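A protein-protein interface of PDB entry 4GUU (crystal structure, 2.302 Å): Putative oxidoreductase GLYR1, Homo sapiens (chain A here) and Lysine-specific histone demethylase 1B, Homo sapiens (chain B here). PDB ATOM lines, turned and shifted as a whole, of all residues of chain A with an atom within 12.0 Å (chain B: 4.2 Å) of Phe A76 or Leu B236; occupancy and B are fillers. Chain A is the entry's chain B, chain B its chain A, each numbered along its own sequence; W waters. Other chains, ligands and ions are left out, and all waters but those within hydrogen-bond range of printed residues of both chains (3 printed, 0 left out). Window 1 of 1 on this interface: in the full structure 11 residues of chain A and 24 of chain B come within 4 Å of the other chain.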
ATOM      1  N   ASP A  70     -18.025  30.309  14.358  1.00  0.00           N
ATOM      2  CA  ASP A  70     -17.480  29.049  14.845  1.00  0.00           C
ATOM      3  C   ASP A  70     -18.141  28.612  16.151  1.00  0.00           C
ATOM      4  O   ASP A  70     -17.874  29.187  17.207  1.00  0.00           O
ATOM      5  CB  ASP A  70     -15.956  29.141  15.009  1.00  0.00           C
ATOM      6  CG  ASP A  70     -15.501  30.492  15.543  1.00  0.00           C
ATOM      7  OD1 ASP A  70     -16.345  31.239  16.082  1.00  0.00           O
ATOM      8  OD2 ASP A  70     -14.296  30.809  15.420  1.00  0.00           O
ATOM      9  N   PRO A  71     -19.006  27.584  16.075  1.00  0.00           N
ATOM     10  CA  PRO A  71     -19.708  26.951  17.198  1.00  0.00           C
ATOM     11  C   PRO A  71     -18.761  26.272  18.191  1.00  0.00           C
ATOM     12  O   PRO A  71     -19.195  25.431  18.980  1.00  0.00           O
ATOM     13  CB  PRO A  71     -20.589  25.902  16.509  1.00  0.00           C
ATOM     14  CG  PRO A  71     -20.751  26.402  15.110  1.00  0.00           C
ATOM     15  CD  PRO A  71     -19.435  27.022  14.783  1.00  0.00           C
ATOM     16  N   HIS A  72     -17.480  26.629  18.137  1.00  0.00           N
ATOM     17  CA  HIS A  72     -16.507  26.185  19.125  1.00  0.00           C
ATOM     18  C   HIS A  72     -16.411  27.314  20.139  1.00  0.00           C
ATOM     19  O   HIS A  72     -15.571  27.308  21.040  1.00  0.00           O
ATOM     20  CB  HIS A  72     -15.153  25.931  18.464  1.00  0.00           C
ATOM     21  CG  HIS A  72     -15.247  25.203  17.152  1.00  0.00           C
ATOM     22  ND1 HIS A  72     -14.701  23.971  16.951  1.00  0.00           N
ATOM     23  CD2 HIS A  72     -15.852  25.567  15.990  1.00  0.00           C
ATOM     24  CE1 HIS A  72     -14.954  23.580  15.698  1.00  0.00           C
ATOM     25  NE2 HIS A  72     -15.644  24.526  15.110  1.00  0.00           N
ATOM     26  N   PHE A  73     -17.295  28.293  19.960  1.00  0.00           N
ATOM     27  CA  PHE A  73     -17.367  29.476  20.807  1.00  0.00           C
ATOM     28  C   PHE A  73     -18.808  29.752  21.233  1.00  0.00           C
ATOM     29  O   PHE A  73     -19.058  30.170  22.361  1.00  0.00           O
ATOM     30  CB  PHE A  73     -16.850  30.703  20.048  1.00  0.00           C
ATOM     31  CG  PHE A  73     -15.355  30.750  19.905  1.00  0.00           C
ATOM     32  CD1 PHE A  73     -14.605  31.641  20.656  1.00  0.00           C
ATOM     33  CD2 PHE A  73     -14.701  29.913  19.019  1.00  0.00           C
ATOM     34  CE1 PHE A  73     -13.232  31.689  20.527  1.00  0.00           C
ATOM     35  CE2 PHE A  73     -13.330  29.956  18.886  1.00  0.00           C
ATOM     36  CZ  PHE A  73     -12.593  30.844  19.642  1.00  0.00           C
ATOM     37  N   HIS A  74     -19.742  29.508  20.316  1.00  0.00           N
ATOM     38  CA  HIS A  74     -21.137  29.933  20.462  1.00  0.00           C
ATOM     39  C   HIS A  74     -21.835  29.426  21.726  1.00  0.00           C
ATOM     40  O   HIS A  74     -21.756  28.244  22.062  1.00  0.00           O
ATOM     41  CB  HIS A  74     -21.939  29.548  19.211  1.00  0.00           C
ATOM     42  CG  HIS A  74     -21.605  30.374  18.003  1.00  0.00           C
ATOM     43  ND1 HIS A  74     -20.851  31.525  18.082  1.00  0.00           N
ATOM     44  CD2 HIS A  74     -21.923  30.213  16.699  1.00  0.00           C
ATOM     45  CE1 HIS A  74     -20.719  32.040  16.871  1.00  0.00           C
ATOM     46  NE2 HIS A  74     -21.358  31.267  16.015  1.00  0.00           N
ATOM     47  N   HIS A  75     -22.523  30.336  22.417  1.00  0.00           N
ATOM     48  CA  HIS A  75     -23.259  30.004  23.636  1.00  0.00           C
ATOM     49  C   HIS A  75     -24.372  29.005  23.349  1.00  0.00           C
ATOM     50  O   HIS A  75     -25.242  29.249  22.514  1.00  0.00           O
ATOM     51  CB  HIS A  75     -23.845  31.261  24.289  1.00  0.00           C
ATOM     52  CG  HIS A  75     -24.330  31.050  25.697  1.00  0.00           C
ATOM     53  ND1 HIS A  75     -25.393  30.218  26.000  1.00  0.00           N
ATOM     54  CD2 HIS A  75     -23.901  31.560  26.869  1.00  0.00           C
ATOM     55  CE1 HIS A  75     -25.589  30.229  27.307  1.00  0.00           C
ATOM     56  NE2 HIS A  75     -24.703  31.031  27.862  1.00  0.00           N
ATOM     57  N   PHE A  76     -24.328  27.880  24.054  1.00  0.00           N
ATOM     58  CA  PHE A  76     -25.299  26.801  23.893  1.00  0.00           C
ATOM     59  C   PHE A  76     -26.755  27.270  23.969  1.00  0.00           C
ATOM     60  O   PHE A  76     -27.606  26.803  23.212  1.00  0.00           O
ATOM     61  CB  PHE A  76     -25.032  25.717  24.944  1.00  0.00           C
ATOM     62  CG  PHE A  76     -26.046  24.609  24.959  1.00  0.00           C
ATOM     63  CD1 PHE A  76     -26.088  23.676  23.940  1.00  0.00           C
ATOM     64  CD2 PHE A  76     -26.942  24.488  26.008  1.00  0.00           C
ATOM     65  CE1 PHE A  76     -27.018  22.647  23.959  1.00  0.00           C
ATOM     66  CE2 PHE A  76     -27.866  23.464  26.037  1.00  0.00           C
ATOM     67  CZ  PHE A  76     -27.908  22.542  25.011  1.00  0.00           C
ATOM     68  N   LEU A  77     -27.039  28.201  24.874  1.00  0.00           N
ATOM     69  CA  LEU A  77     -28.420  28.616  25.117  1.00  0.00           C
ATOM     70  C   LEU A  77     -28.919  29.688  24.148  1.00  0.00           C
ATOM     71  O   LEU A  77     -30.125  29.904  24.018  1.00  0.00           O
ATOM     72  CB  LEU A  77     -28.603  29.069  26.569  1.00  0.00           C
ATOM     73  CG  LEU A  77     -28.540  27.950  27.614  1.00  0.00           C
ATOM     74  CD1 LEU A  77     -28.691  28.516  29.018  1.00  0.00           C
ATOM     75  CD2 LEU A  77     -29.599  26.886  27.339  1.00  0.00           C
ATOM     76  N   LEU A  78     -27.990  30.353  23.470  1.00  0.00           N
ATOM     77  CA  LEU A  78     -28.349  31.353  22.472  1.00  0.00           C
ATOM     78  C   LEU A  78     -28.009  30.866  21.060  1.00  0.00           C
ATOM     79  O   LEU A  78     -27.700  31.664  20.174  1.00  0.00           O
ATOM     80  CB  LEU A  78     -27.658  32.686  22.772  1.00  0.00           C
ATOM     81  CG  LEU A  78     -28.060  33.331  24.104  1.00  0.00           C
ATOM     82  CD1 LEU A  78     -27.248  34.585  24.378  1.00  0.00           C
ATOM     83  CD2 LEU A  78     -29.552  33.644  24.118  1.00  0.00           C
ATOM     84  N   SER A  79     -28.075  29.551  20.863  1.00  0.00           N
ATOM     85  CA  SER A  79     -27.813  28.949  19.557  1.00  0.00           C
ATOM     86  C   SER A  79     -28.892  27.934  19.184  1.00  0.00           C
ATOM     87  O   SER A  79     -28.650  27.031  18.383  1.00  0.00           O
ATOM     88  CB  SER A  79     -26.447  28.255  19.545  1.00  0.00           C
ATOM     89  OG  SER A  79     -25.403  29.160  19.853  1.00  0.00           O
ATOM     90  N   GLN A  80     -30.083  28.089  19.757  1.00  0.00           N
ATOM     91  CA  GLN A  80     -31.146  27.099  19.600  1.00  0.00           C
ATOM     92  C   GLN A  80     -32.093  27.352  18.424  1.00  0.00           C
ATOM     93  O   GLN A  80     -33.082  26.639  18.254  1.00  0.00           O
ATOM     94  CB  GLN A  80     -31.946  26.965  20.898  1.00  0.00           C
ATOM     95  CG  GLN A  80     -31.164  26.332  22.031  1.00  0.00           C
ATOM     96  CD  GLN A  80     -30.745  24.908  21.729  1.00  0.00           C
ATOM     97  OE1 GLN A  80     -31.384  24.213  20.938  1.00  0.00           O
ATOM     98  NE2 GLN A  80     -29.655  24.468  22.348  1.00  0.00           N
ATOM     99  N   THR A  81     -31.794  28.364  17.616  1.00  0.00           N
ATOM    100  CA  THR A  81     -32.578  28.620  16.410  1.00  0.00           C
ATOM    101  C   THR A  81     -31.762  28.316  15.152  1.00  0.00           C
ATOM    102  O   THR A  81     -30.734  27.637  15.216  1.00  0.00           O
ATOM    103  CB  THR A  81     -33.093  30.074  16.355  1.00  0.00           C
ATOM    104  OG1 THR A  81     -31.984  30.978  16.261  1.00  0.00           O
ATOM    105  CG2 THR A  81     -33.915  30.404  17.597  1.00  0.00           C
ATOM    106  N   LYS B 234     -15.013  28.403  25.256  1.00  0.00           N
ATOM    107  CA  LYS B 234     -15.418  27.707  26.470  1.00  0.00           C
ATOM    108  C   LYS B 234     -16.928  27.818  26.678  1.00  0.00           C
ATOM    109  O   LYS B 234     -17.561  28.763  26.207  1.00  0.00           O
ATOM    110  CB  LYS B 234     -14.650  28.207  27.695  1.00  0.00           C
ATOM    111  CG  LYS B 234     -14.966  29.623  28.140  1.00  0.00           C
ATOM    112  CD  LYS B 234     -14.205  29.924  29.414  1.00  0.00           C
ATOM    113  CE  LYS B 234     -14.065  31.408  29.673  1.00  0.00           C
ATOM    114  NZ  LYS B 234     -13.041  31.645  30.727  1.00  0.00           N
ATOM    115  N   ALA B 235     -17.488  26.842  27.387  1.00  0.00           N
ATOM    116  CA  ALA B 235     -18.935  26.664  27.489  1.00  0.00           C
ATOM    117  C   ALA B 235     -19.654  27.826  28.155  1.00  0.00           C
ATOM    118  O   ALA B 235     -19.144  28.426  29.101  1.00  0.00           O
ATOM    119  CB  ALA B 235     -19.255  25.375  28.223  1.00  0.00           C
ATOM    120  N   LEU B 236     -20.849  28.124  27.650  1.00  0.00           N
ATOM    121  CA  LEU B 236     -21.710  29.163  28.206  1.00  0.00           C
ATOM    122  C   LEU B 236     -20.994  30.504  28.339  1.00  0.00           C
ATOM    123  O   LEU B 236     -21.085  31.173  29.370  1.00  0.00           O
ATOM    124  CB  LEU B 236     -22.296  28.724  29.552  1.00  0.00           C
ATOM    125  CG  LEU B 236     -23.074  27.401  29.562  1.00  0.00           C
ATOM    126  CD1 LEU B 236     -23.983  27.323  30.781  1.00  0.00           C
ATOM    127  CD2 LEU B 236     -23.888  27.227  28.291  1.00  0.00           C
ATOM    128  N   CYS B 237     -20.286  30.889  27.284  1.00  0.00           N
ATOM    129  CA  CYS B 237     -19.577  32.155  27.261  1.00  0.00           C
ATOM    130  C   CYS B 237     -20.092  32.978  26.091  1.00  0.00           C
ATOM    131  O   CYS B 237     -20.357  32.431  25.022  1.00  0.00           O
ATOM    132  CB  CYS B 237     -18.081  31.901  27.103  1.00  0.00           C
ATOM    133  SG  CYS B 237     -17.024  33.148  27.849  1.00  0.00           S
ATOM    134  N   ASN B 398     -18.474  28.739  34.564  1.00  0.00           N
ATOM    135  CA  ASN B 398     -19.742  28.937  33.868  1.00  0.00           C
ATOM    136  C   ASN B 398     -20.691  27.743  33.984  1.00  0.00           C
ATOM    137  O   ASN B 398     -21.721  27.691  33.316  1.00  0.00           O
ATOM    138  CB  ASN B 398     -19.508  29.306  32.399  1.00  0.00           C
ATOM    139  CG  ASN B 398     -18.731  30.606  32.239  1.00  0.00           C
ATOM    140  OD1 ASN B 398     -18.679  31.427  33.159  1.00  0.00           O
ATOM    141  ND2 ASN B 398     -18.126  30.798  31.071  1.00  0.00           N
ATOM    142  N   PRO B 400     -23.586  25.638  35.413  1.00  0.00           N
ATOM    143  CA  PRO B 400     -24.820  25.882  36.171  1.00  0.00           C
ATOM    144  C   PRO B 400     -24.741  25.246  37.554  1.00  0.00           C
ATOM    145  O   PRO B 400     -25.306  25.768  38.515  1.00  0.00           O
ATOM    146  CB  PRO B 400     -25.890  25.168  35.338  1.00  0.00           C
ATOM    147  CG  PRO B 400     -25.321  25.104  33.968  1.00  0.00           C
ATOM    148  CD  PRO B 400     -23.851  24.909  34.162  1.00  0.00           C
ATOM    149  N   PHE B 522     -16.717  22.932  29.178  1.00  0.00           N
ATOM    150  CA  PHE B 522     -16.593  23.656  30.438  1.00  0.00           C
ATOM    151  C   PHE B 522     -15.145  23.686  30.920  1.00  0.00           C
ATOM    152  O   PHE B 522     -14.510  22.645  31.091  1.00  0.00           O
ATOM    153  CB  PHE B 522     -17.524  23.073  31.509  1.00  0.00           C
ATOM    154  CG  PHE B 522     -18.981  23.368  31.268  1.00  0.00           C
ATOM    155  CD1 PHE B 522     -19.786  22.457  30.605  1.00  0.00           C
ATOM    156  CD2 PHE B 522     -19.539  24.568  31.688  1.00  0.00           C
ATOM    157  CE1 PHE B 522     -21.118  22.732  30.369  1.00  0.00           C
ATOM    158  CE2 PHE B 522     -20.876  24.849  31.458  1.00  0.00           C
ATOM    159  CZ  PHE B 522     -21.667  23.930  30.797  1.00  0.00           C
ATOM    160  N   ASN B 752     -28.520  16.035  24.701  1.00  0.00           N
ATOM    161  CA  ASN B 752     -27.613  17.181  24.698  1.00  0.00           C
ATOM    162  C   ASN B 752     -26.317  16.872  23.950  1.00  0.00           C
ATOM    163  O   ASN B 752     -25.463  16.143  24.448  1.00  0.00           O
ATOM    164  CB  ASN B 752     -27.300  17.629  26.128  1.00  0.00           C
ATOM    165  CG  ASN B 752     -26.695  19.027  26.182  1.00  0.00           C
ATOM    166  OD1 ASN B 752     -25.919  19.415  25.308  1.00  0.00           O
ATOM    167  ND2 ASN B 752     -27.055  19.789  27.207  1.00  0.00           N
ATOM    168  N   HIS B 754     -23.883  19.045  22.824  1.00  0.00           N
ATOM    169  CA  HIS B 754     -22.720  19.777  23.311  1.00  0.00           C
ATOM    170  C   HIS B 754     -22.179  19.146  24.578  1.00  0.00           C
ATOM    171  O   HIS B 754     -20.969  19.015  24.750  1.00  0.00           O
ATOM    172  CB  HIS B 754     -23.092  21.229  23.600  1.00  0.00           C
ATOM    173  CG  HIS B 754     -23.391  22.028  22.376  1.00  0.00           C
ATOM    174  ND1 HIS B 754     -22.643  23.125  22.007  1.00  0.00           N
ATOM    175  CD2 HIS B 754     -24.358  21.897  21.436  1.00  0.00           C
ATOM    176  CE1 HIS B 754     -23.138  23.636  20.893  1.00  0.00           C
ATOM    177  NE2 HIS B 754     -24.175  22.909  20.526  1.00  0.00           N
ATOM    178  N   PHE B 755     -23.097  18.764  25.465  1.00  0.00           N
ATOM    179  CA  PHE B 755     -22.748  18.250  26.784  1.00  0.00           C
ATOM    180  C   PHE B 755     -23.513  16.976  27.110  1.00  0.00           C
ATOM    181  O   PHE B 755     -24.386  16.967  27.989  1.00  0.00           O
ATOM    182  CB  PHE B 755     -23.002  19.318  27.846  1.00  0.00           C
ATOM    183  CG  PHE B 755     -22.594  20.703  27.417  1.00  0.00           C
ATOM    184  CD1 PHE B 755     -21.257  21.024  27.234  1.00  0.00           C
ATOM    185  CD2 PHE B 755     -23.550  21.682  27.199  1.00  0.00           C
ATOM    186  CE1 PHE B 755     -20.882  22.295  26.836  1.00  0.00           C
ATOM    187  CE2 PHE B 755     -23.182  22.954  26.803  1.00  0.00           C
ATOM    188  CZ  PHE B 755     -21.847  23.262  26.621  1.00  0.00           C
ATOM    189  N   LEU B 764     -29.057  21.358  31.575  1.00  0.00           N
ATOM    190  CA  LEU B 764     -29.111  22.345  30.496  1.00  0.00           C
ATOM    191  C   LEU B 764     -30.118  21.969  29.402  1.00  0.00           C
ATOM    192  O   LEU B 764     -30.717  22.841  28.775  1.00  0.00           O
ATOM    193  CB  LEU B 764     -27.719  22.582  29.901  1.00  0.00           C
ATOM    194  CG  LEU B 764     -26.736  23.386  30.761  1.00  0.00           C
ATOM    195  CD1 LEU B 764     -25.310  23.246  30.253  1.00  0.00           C
ATOM    196  CD2 LEU B 764     -27.140  24.850  30.804  1.00  0.00           C
HETATM  197  O   HOH W   1     -21.395  27.155  25.144  1.00  0.00           O
HETATM  198  O   HOH W   2     -20.609  32.696  22.332  1.00  0.00           O
HETATM  199  O   HOH W   3     -19.830  29.385  24.758  1.00  0.00           O
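The backbone NH (N) of His B754 sits at hydrogen-bond distance from the side-chain amide oxygen (OD1) of Asn B752, 3.2 Å away. OG of Ser A79 sits at hydrogen-bond distance from O of His A75. The backbone NH of Leu A77 is in hydrogen-bond range of a ring nitrogen (ND1) of His A75 (2.8 Å). The backbone carbonyl oxygen (O) of Leu B236 sits at hydrogen-bond distance from the side-chain amide nitrogen (ND2) of Asn B398 (3.4 Å). O of Phe A76 sits at hydrogen-bond distance from NE2 of Gln A80 (3.2 Å). The backbone NH (N) of Phe B755 is in hydrogen-bond range of the side-chain amide oxygen (OD1) of Asn B752, 2.9 Å away.
Among the printed residues, pairs that only touch across the chains: His A75 with Leu B236, Phe A76 with His B754, Phe A76 with Asn B752, His A75 with Cys B237, Phe A73 with Cys B237, Phe A76 with Phe B755, Phe A76 with Leu B236 and Phe A76 with Leu B764.
Phe A76 touches five residues of chain B. Leu B236 touches just these residues of chain A: His A75 and Phe A76. Of chain A, only Phe A73 (3.7 Å) and His A75 (3.7 Å) come within 4 Å of Cys B237. No residue of chain A comes within 4 Å of Asn B398. Of chain A, only Phe A76 (3.6 Å) comes within 4 Å of Asn B752. Printed residues of chain A within 4 Å of Phe B755: Phe A76. Of the printed residues of chain A, Leu B764 touches Phe A76. Printed residues of chain B within 4 Å of His A75: Leu B236 and Cys B237. Of the printed residues of chain B, Phe A73 touches Cys B237. Lys B234 touches none of the printed residues of chain A. Pro A71 touches none of the printed residues of chain B. The nearest residue of chain A that does not touch Leu B236 is Leu A77 (4.7 Å).
Of the 11 printed residues of chain B, 6 touch a printed residue of chain A. Printed residues of chain B that touch a printed residue of chain A: Leu B236, Cys B237, Asn B752, His B754, Phe B755 and Leu B764. Of the 12 printed residues of chain A, 3 touch a printed residue of chain B. Among the printed residues, 8 pairs touch across the chains. Among the printed residues, no Asp or Glu carboxylate lies within 4 Å of a Lys or Arg side-chain nitrogen of the other chain.
Water W3 lies within hydrogen-bond range of the backbone carbonyl oxygen of Phe A73 (2.6 Å), the backbone carbonyl oxygen of Lys B234 (2.8 Å), the backbone NH of Cys B237 (3.0 Å) and the backbone NH of Leu B236 (3.3 Å). Water W2 lies within hydrogen-bond range of O of Cys B237 (2.7 Å), O of Phe A73 (3.0 Å) and N of His A75 (3.0 Å). Water W1 lies within hydrogen-bond range of the backbone NH of Leu B236 (2.7 Å), the backbone NH of Phe A76 (3.2 Å) and the backbone carbonyl oxygen of His A74 (3.3 Å).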
